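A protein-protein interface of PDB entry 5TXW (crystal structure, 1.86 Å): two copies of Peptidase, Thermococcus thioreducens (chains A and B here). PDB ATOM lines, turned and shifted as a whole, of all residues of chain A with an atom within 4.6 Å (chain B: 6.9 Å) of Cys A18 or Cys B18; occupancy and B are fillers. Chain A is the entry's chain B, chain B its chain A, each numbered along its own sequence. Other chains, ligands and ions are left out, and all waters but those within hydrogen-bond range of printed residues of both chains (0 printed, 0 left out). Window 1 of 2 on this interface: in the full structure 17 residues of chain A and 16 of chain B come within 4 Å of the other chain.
SG of Cys B18 forms a disulfide with SG of Cys A18 (2.1 Å).
The guanidinium group (NE) of Arg A22 lies close to the guanidinium group (NE) of Arg B22 (3.5 Å).
Among the printed residues, pairs that only touch across the chains: Leu A14 with Leu B14, Leu A154 with His B21, His A21 with Leu B154, Ile A17 with Leu B14 and Leu A14 with Ile B17.
Of the printed residues of chain B, Leu A14 touches Leu B14 and Ile B17.
Of the printed residues of chain B, Cys A18 touches Cys B18 (2.1 Å).
Pro A19 touches none of the printed residues of chain B.
Printed residues of chain B within 4 Å of Leu A154: His B21.
Printed residues of chain A within 4 Å of Ile B17: Leu A14.
Printed residues of chain A within 4 Å of Cys B18: Cys A18.
Printed residues of chain A within 4 Å of His B21: Leu A154 (3.6 Å).
Printed residues of chain A within 4 Å of Arg B22: Arg A22.
Ile B23 touches none of the printed residues of chain A.
The nearest printed residue of chain A that does not touch Cys B18 is Leu A14 (4.6 Å).
The nearest printed residue of chain A that does not touch Ile B17 is Cys A18 (4.7 Å).
Of the 9 printed residues of chain A, 6 touch a printed residue of chain B.
Hydrophobic or aromatic side chains of chain A that line the printed part of chain B: Leu A14, Ile A17, His A21 and Leu A154.
Of the 14 printed residues of chain B, 6 touch a printed residue of chain A.
Hydrophobic or aromatic side chains of chain B within 4 Å of the printed part of chain A: Leu B14, Ile B17, His B21 and Leu B154.
Among the printed residues, 7 pairs touch across the chains.
Among the printed residues, no Asp or Glu carboxylate lies within 4 Å of a Lys or Arg side-chain nitrogen of the other chain.
Leu A14 touches its own counterpart, Leu B14.
Leu A14 touches Ile B17, and with the chains exchanged Ile A17 touches Leu B14.
Cys A18 touches its own counterpart, Cys B18.
Arg A22 touches its own counterpart, Arg B22.
Positions printed for both chains: 14, 16, 17, 18, 19, 20, 21, 22 and 154.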
ATOM      1  N   LEU A  14      -7.567 -31.368  -4.778  1.00  0.00           N
ATOM      2  CA  LEU A  14      -6.655 -31.580  -5.915  1.00  0.00           C
ATOM      3  C   LEU A  14      -6.526 -33.062  -6.303  1.00  0.00           C
ATOM      4  O   LEU A  14      -6.230 -33.360  -7.453  1.00  0.00           O
ATOM      5  CB  LEU A  14      -5.260 -31.082  -5.577  1.00  0.00           C
ATOM      6  CG  LEU A  14      -5.108 -29.610  -5.293  1.00  0.00           C
ATOM      7  CD1 LEU A  14      -3.681 -29.356  -4.846  1.00  0.00           C
ATOM      8  CD2 LEU A  14      -5.474 -28.809  -6.530  1.00  0.00           C
ATOM      9  N   LEU A  16      -8.587 -35.368  -6.256  1.00  0.00           N
ATOM     10  CA  LEU A  16      -9.709 -35.858  -7.050  1.00  0.00           C
ATOM     11  C   LEU A  16      -9.825 -35.090  -8.375  1.00  0.00           C
ATOM     12  O   LEU A  16      -9.952 -35.686  -9.462  1.00  0.00           O
ATOM     13  CB  LEU A  16     -10.995 -35.719  -6.222  1.00  0.00           C
ATOM     14  CG  LEU A  16     -12.343 -35.983  -6.889  1.00  0.00           C
ATOM     15  CD1 LEU A  16     -12.411 -37.403  -7.442  1.00  0.00           C
ATOM     16  CD2 LEU A  16     -13.481 -35.720  -5.908  1.00  0.00           C
ATOM     17  N   ILE A  17      -9.750 -33.765  -8.303  1.00  0.00           N
ATOM     18  CA  ILE A  17     -10.098 -32.950  -9.466  1.00  0.00           C
ATOM     19  C   ILE A  17      -8.967 -32.941 -10.536  1.00  0.00           C
ATOM     20  O   ILE A  17      -9.253 -33.047 -11.724  1.00  0.00           O
ATOM     21  CB  ILE A  17     -10.517 -31.528  -9.027  1.00  0.00           C
ATOM     22  CG1 ILE A  17     -11.830 -31.595  -8.238  1.00  0.00           C
ATOM     23  CG2 ILE A  17     -10.741 -30.624 -10.232  1.00  0.00           C
ATOM     24  CD1 ILE A  17     -12.138 -30.330  -7.451  1.00  0.00           C
ATOM     25  N   CYS A  18      -7.695 -32.853 -10.144  1.00  0.00           N
ATOM     26  CA  CYS A  18      -6.637 -32.861 -11.156  1.00  0.00           C
ATOM     27  C   CYS A  18      -6.583 -34.210 -11.936  1.00  0.00           C
ATOM     28  O   CYS A  18      -6.657 -34.187 -13.156  1.00  0.00           O
ATOM     29  CB  CYS A  18      -5.267 -32.459 -10.579  1.00  0.00           C
ATOM     30  SG  CYS A  18      -5.092 -30.774  -9.855  1.00  0.00           S
ATOM     31  N   PRO A  19      -6.733 -35.347 -11.241  1.00  0.00           N
ATOM     32  CA  PRO A  19      -6.812 -36.573 -12.042  1.00  0.00           C
ATOM     33  C   PRO A  19      -8.070 -36.700 -12.888  1.00  0.00           C
ATOM     34  O   PRO A  19      -8.033 -37.308 -13.964  1.00  0.00           O
ATOM     35  CB  PRO A  19      -6.755 -37.682 -10.994  1.00  0.00           C
ATOM     36  CG  PRO A  19      -5.930 -37.099  -9.912  1.00  0.00           C
ATOM     37  CD  PRO A  19      -6.179 -35.613  -9.901  1.00  0.00           C
ATOM     38  N   LEU A  20      -9.187 -36.167 -12.400  1.00  0.00           N
ATOM     39  CA  LEU A  20     -10.409 -36.221 -13.184  1.00  0.00           C
ATOM     40  C   LEU A  20     -10.128 -35.578 -14.552  1.00  0.00           C
ATOM     41  O   LEU A  20     -10.527 -36.105 -15.587  1.00  0.00           O
ATOM     42  CB  LEU A  20     -11.523 -35.438 -12.497  1.00  0.00           C
ATOM     43  CG  LEU A  20     -12.501 -36.179 -11.592  1.00  0.00           C
ATOM     44  CD1 LEU A  20     -13.554 -35.196 -11.095  1.00  0.00           C
ATOM     45  CD2 LEU A  20     -13.131 -37.359 -12.315  1.00  0.00           C
ATOM     46  N   HIS A  21      -9.465 -34.423 -14.541  1.00  0.00           N
ATOM     47  CA  HIS A  21      -9.203 -33.712 -15.778  1.00  0.00           C
ATOM     48  C   HIS A  21      -8.135 -34.419 -16.599  1.00  0.00           C
ATOM     49  O   HIS A  21      -8.178 -34.393 -17.821  1.00  0.00           O
ATOM     50  CB  HIS A  21      -8.803 -32.256 -15.504  1.00  0.00           C
ATOM     51  CG  HIS A  21      -9.974 -31.365 -15.274  1.00  0.00           C
ATOM     52  ND1 HIS A  21     -10.812 -30.985 -16.304  1.00  0.00           N
ATOM     53  CD2 HIS A  21     -10.610 -31.014 -14.131  1.00  0.00           C
ATOM     54  CE1 HIS A  21     -11.792 -30.247 -15.810  1.00  0.00           C
ATOM     55  NE2 HIS A  21     -11.766 -30.361 -14.497  1.00  0.00           N
ATOM     56  N   ARG A  22      -7.106 -34.928 -15.930  1.00  0.00           N
ATOM     57  CA  ARG A  22      -6.000 -35.566 -16.618  1.00  0.00           C
ATOM     58  C   ARG A  22      -6.494 -36.769 -17.417  1.00  0.00           C
ATOM     59  O   ARG A  22      -6.072 -37.005 -18.553  1.00  0.00           O
ATOM     60  CB  ARG A  22      -4.955 -36.029 -15.625  1.00  0.00           C
ATOM     61  CG  ARG A  22      -3.794 -36.721 -16.294  1.00  0.00           C
ATOM     62  CD  ARG A  22      -2.940 -35.721 -17.021  1.00  0.00           C
ATOM     63  NE  ARG A  22      -1.893 -36.369 -17.783  1.00  0.00           N
ATOM     64  CZ  ARG A  22      -2.071 -36.928 -18.972  1.00  0.00           C
ATOM     65  NH1 ARG A  22      -3.273 -37.030 -19.509  1.00  0.00           N
ATOM     66  NH2 ARG A  22      -1.057 -37.539 -19.545  1.00  0.00           N
ATOM     67  N   LEU A 154       1.570 -35.376  -7.294  1.00  0.00           N
ATOM     68  CA  LEU A 154       0.579 -35.598  -8.335  1.00  0.00           C
ATOM     69  C   LEU A 154       1.183 -35.909  -9.721  1.00  0.00           C
ATOM     70  O   LEU A 154       0.647 -36.746 -10.442  1.00  0.00           O
ATOM     71  CB  LEU A 154      -0.380 -34.412  -8.475  1.00  0.00           C
ATOM     72  CG  LEU A 154      -1.519 -34.271  -7.464  1.00  0.00           C
ATOM     73  CD1 LEU A 154      -2.168 -32.914  -7.646  1.00  0.00           C
ATOM     74  CD2 LEU A 154      -2.551 -35.371  -7.641  1.00  0.00           C
ATOM     75  N   PHE B   5       5.184 -19.656 -15.099  1.00  0.00           N
ATOM     76  CA  PHE B   5       3.875 -19.247 -14.610  1.00  0.00           C
ATOM     77  C   PHE B   5       4.009 -17.885 -13.915  1.00  0.00           C
ATOM     78  O   PHE B   5       4.879 -17.690 -13.080  1.00  0.00           O
ATOM     79  CB  PHE B   5       3.329 -20.254 -13.600  1.00  0.00           C
ATOM     80  CG  PHE B   5       2.910 -21.572 -14.202  1.00  0.00           C
ATOM     81  CD1 PHE B   5       3.857 -22.455 -14.682  1.00  0.00           C
ATOM     82  CD2 PHE B   5       1.606 -22.023 -14.056  1.00  0.00           C
ATOM     83  CE1 PHE B   5       3.486 -23.656 -15.251  1.00  0.00           C
ATOM     84  CE2 PHE B   5       1.238 -23.267 -14.561  1.00  0.00           C
ATOM     85  CZ  PHE B   5       2.167 -24.041 -15.233  1.00  0.00           C
ATOM     86  N   ASP B  13      -6.942 -21.700  -7.428  1.00  0.00           N
ATOM     87  CA  ASP B  13      -6.005 -22.769  -7.052  1.00  0.00           C
ATOM     88  C   ASP B  13      -5.860 -23.818  -8.153  1.00  0.00           C
ATOM     89  O   ASP B  13      -4.758 -24.181  -8.523  1.00  0.00           O
ATOM     90  CB  ASP B  13      -6.474 -23.458  -5.763  1.00  0.00           C
ATOM     91  CG  ASP B  13      -6.702 -22.495  -4.630  1.00  0.00           C
ATOM     92  OD1 ASP B  13      -7.485 -21.537  -4.824  1.00  0.00           O
ATOM     93  OD2 ASP B  13      -6.158 -22.706  -3.522  1.00  0.00           O
ATOM     94  N   LEU B  14      -6.959 -24.333  -8.678  1.00  0.00           N
ATOM     95  CA  LEU B  14      -6.865 -25.415  -9.667  1.00  0.00           C
ATOM     96  C   LEU B  14      -6.178 -24.966 -10.952  1.00  0.00           C
ATOM     97  O   LEU B  14      -5.616 -25.786 -11.687  1.00  0.00           O
ATOM     98  CB  LEU B  14      -8.255 -25.936 -10.025  1.00  0.00           C
ATOM     99  CG  LEU B  14      -9.014 -26.654  -8.926  1.00  0.00           C
ATOM    100  CD1 LEU B  14     -10.417 -26.945  -9.423  1.00  0.00           C
ATOM    101  CD2 LEU B  14      -8.340 -27.965  -8.575  1.00  0.00           C
ATOM    102  N   GLU B  15      -6.429 -23.708 -11.326  1.00  0.00           N
ATOM    103  CA  GLU B  15      -5.953 -23.158 -12.592  1.00  0.00           C
ATOM    104  C   GLU B  15      -4.439 -22.991 -12.602  1.00  0.00           C
ATOM    105  O   GLU B  15      -3.833 -22.942 -13.672  1.00  0.00           O
ATOM    106  CB  GLU B  15      -6.637 -21.814 -12.867  1.00  0.00           C
ATOM    107  CG  GLU B  15      -8.104 -21.958 -13.268  1.00  0.00           C
ATOM    108  CD  GLU B  15      -8.805 -20.625 -13.426  1.00  0.00           C
ATOM    109  OE1 GLU B  15      -8.112 -19.599 -13.345  1.00  0.00           O
ATOM    110  OE2 GLU B  15     -10.061 -20.595 -13.423  1.00  0.00           O
ATOM    111  N   LEU B  16      -3.820 -22.917 -11.420  1.00  0.00           N
ATOM    112  CA  LEU B  16      -2.368 -22.889 -11.332  1.00  0.00           C
ATOM    113  C   LEU B  16      -1.836 -24.280 -11.041  1.00  0.00           C
ATOM    114  O   LEU B  16      -0.949 -24.751 -11.717  1.00  0.00           O
ATOM    115  CB  LEU B  16      -1.909 -21.907 -10.250  1.00  0.00           C
ATOM    116  CG  LEU B  16      -0.418 -21.910  -9.888  1.00  0.00           C
ATOM    117  CD1 LEU B  16       0.472 -21.674 -11.096  1.00  0.00           C
ATOM    118  CD2 LEU B  16      -0.087 -20.889  -8.802  1.00  0.00           C
ATOM    119  N   ILE B  17      -2.443 -24.980 -10.097  1.00  0.00           N
ATOM    120  CA  ILE B  17      -1.833 -26.188  -9.594  1.00  0.00           C
ATOM    121  C   ILE B  17      -1.983 -27.369 -10.545  1.00  0.00           C
ATOM    122  O   ILE B  17      -1.001 -28.072 -10.758  1.00  0.00           O
ATOM    123  CB  ILE B  17      -2.315 -26.548  -8.189  1.00  0.00           C
ATOM    124  CG1 ILE B  17      -1.823 -25.464  -7.217  1.00  0.00           C
ATOM    125  CG2 ILE B  17      -1.754 -27.914  -7.818  1.00  0.00           C
ATOM    126  CD1 ILE B  17      -2.437 -25.494  -5.827  1.00  0.00           C
ATOM    127  N   CYS B  18      -3.155 -27.563 -11.161  1.00  0.00           N
ATOM    128  CA  CYS B  18      -3.320 -28.729 -12.048  1.00  0.00           C
ATOM    129  C   CYS B  18      -2.393 -28.633 -13.295  1.00  0.00           C
ATOM    130  O   CYS B  18      -1.701 -29.603 -13.616  1.00  0.00           O
ATOM    131  CB  CYS B  18      -4.795 -28.966 -12.442  1.00  0.00           C
ATOM    132  SG  CYS B  18      -5.980 -29.404 -11.107  1.00  0.00           S
ATOM    133  N   PRO B  19      -2.253 -27.436 -13.894  1.00  0.00           N
ATOM    134  CA  PRO B  19      -1.296 -27.337 -15.010  1.00  0.00           C
ATOM    135  C   PRO B  19       0.153 -27.486 -14.616  1.00  0.00           C
ATOM    136  O   PRO B  19       0.932 -28.041 -15.377  1.00  0.00           O
ATOM    137  CB  PRO B  19      -1.542 -25.929 -15.545  1.00  0.00           C
ATOM    138  CG  PRO B  19      -2.975 -25.674 -15.242  1.00  0.00           C
ATOM    139  CD  PRO B  19      -3.171 -26.277 -13.878  1.00  0.00           C
ATOM    140  N   LEU B  20       0.529 -26.985 -13.446  1.00  0.00           N
ATOM    141  CA  LEU B  20       1.888 -27.154 -12.971  1.00  0.00           C
ATOM    142  C   LEU B  20       2.258 -28.639 -12.956  1.00  0.00           C
ATOM    143  O   LEU B  20       3.309 -29.033 -13.448  1.00  0.00           O
ATOM    144  CB  LEU B  20       1.987 -26.652 -11.540  1.00  0.00           C
ATOM    145  CG  LEU B  20       2.543 -25.269 -11.280  1.00  0.00           C
ATOM    146  CD1 LEU B  20       2.596 -25.090  -9.766  1.00  0.00           C
ATOM    147  CD2 LEU B  20       3.916 -25.108 -11.912  1.00  0.00           C
ATOM    148  N   HIS B  21       1.379 -29.466 -12.408  1.00  0.00           N
ATOM    149  CA  HIS B  21       1.658 -30.906 -12.345  1.00  0.00           C
ATOM    150  C   HIS B  21       1.572 -31.540 -13.725  1.00  0.00           C
ATOM    151  O   HIS B  21       2.324 -32.442 -14.030  1.00  0.00           O
ATOM    152  CB  HIS B  21       0.717 -31.610 -11.362  1.00  0.00           C
ATOM    153  CG  HIS B  21       1.133 -31.446  -9.946  1.00  0.00           C
ATOM    154  ND1 HIS B  21       2.288 -32.025  -9.467  1.00  0.00           N
ATOM    155  CD2 HIS B  21       0.776 -30.523  -9.027  1.00  0.00           C
ATOM    156  CE1 HIS B  21       2.541 -31.572  -8.257  1.00  0.00           C
ATOM    157  NE2 HIS B  21       1.642 -30.653  -7.967  1.00  0.00           N
ATOM    158  N   ARG B  22       0.601 -31.125 -14.529  1.00  0.00           N
ATOM    159  CA  ARG B  22       0.471 -31.673 -15.876  1.00  0.00           C
ATOM    160  C   ARG B  22       1.754 -31.480 -16.674  1.00  0.00           C
ATOM    161  O   ARG B  22       2.168 -32.338 -17.450  1.00  0.00           O
ATOM    162  CB  ARG B  22      -0.684 -31.023 -16.640  1.00  0.00           C
ATOM    163  CG  ARG B  22      -0.786 -31.494 -18.080  1.00  0.00           C
ATOM    164  CD  ARG B  22      -1.465 -32.847 -18.145  1.00  0.00           C
ATOM    165  NE  ARG B  22      -1.543 -33.363 -19.497  1.00  0.00           N
ATOM    166  CZ  ARG B  22      -0.545 -33.971 -20.132  1.00  0.00           C
ATOM    167  NH1 ARG B  22       0.650 -34.097 -19.574  1.00  0.00           N
ATOM    168  NH2 ARG B  22      -0.751 -34.430 -21.350  1.00  0.00           N
ATOM    169  N   ILE B  23       2.314 -30.297 -16.576  1.00  0.00           N
ATOM    170  CA  ILE B  23       3.466 -29.960 -17.400  1.00  0.00           C
ATOM    171  C   ILE B  23       4.762 -30.593 -16.863  1.00  0.00           C
ATOM    172  O   ILE B  23       5.600 -31.055 -17.658  1.00  0.00           O
ATOM    173  CB  ILE B  23       3.577 -28.431 -17.546  1.00  0.00           C
ATOM    174  CG1 ILE B  23       2.416 -27.934 -18.415  1.00  0.00           C
ATOM    175  CG2 ILE B  23       4.917 -28.022 -18.137  1.00  0.00           C
ATOM    176  CD1 ILE B  23       2.207 -26.437 -18.346  1.00  0.00           C
ATOM    177  N   LEU B 154     -10.452 -27.205 -17.916  1.00  0.00           N
ATOM    178  CA  LEU B 154      -9.039 -27.516 -17.744  1.00  0.00           C
ATOM    179  C   LEU B 154      -8.556 -28.625 -18.684  1.00  0.00           C
ATOM    180  O   LEU B 154      -7.423 -28.572 -19.148  1.00  0.00           O
ATOM    181  CB  LEU B 154      -8.720 -27.910 -16.295  1.00  0.00           C
ATOM    182  CG  LEU B 154      -8.448 -26.792 -15.291  1.00  0.00           C
ATOM    183  CD1 LEU B 154      -8.476 -27.337 -13.865  1.00  0.00           C
ATOM    184  CD2 LEU B 154      -7.111 -26.119 -15.580  1.00  0.00           C
ATOM    185  N   MET B 158      -5.415 -27.864 -21.310  1.00  0.00           N
ATOM    186  CA  MET B 158      -4.154 -28.538 -21.237  1.00  0.00           C
ATOM    187  C   MET B 158      -3.910 -29.451 -22.435  1.00  0.00           C
ATOM    188  O   MET B 158      -2.799 -29.504 -22.956  1.00  0.00           O
ATOM    189  CB  MET B 158      -3.996 -29.273 -19.909  1.00  0.00           C
ATOM    190  CG  MET B 158      -3.607 -28.339 -18.769  1.00  0.00           C
ATOM    191  SD  MET B 158      -2.034 -27.484 -18.970  1.00  0.00           S
ATOM    192  CE  MET B 158      -2.496 -25.852 -19.517  1.00  0.00           C
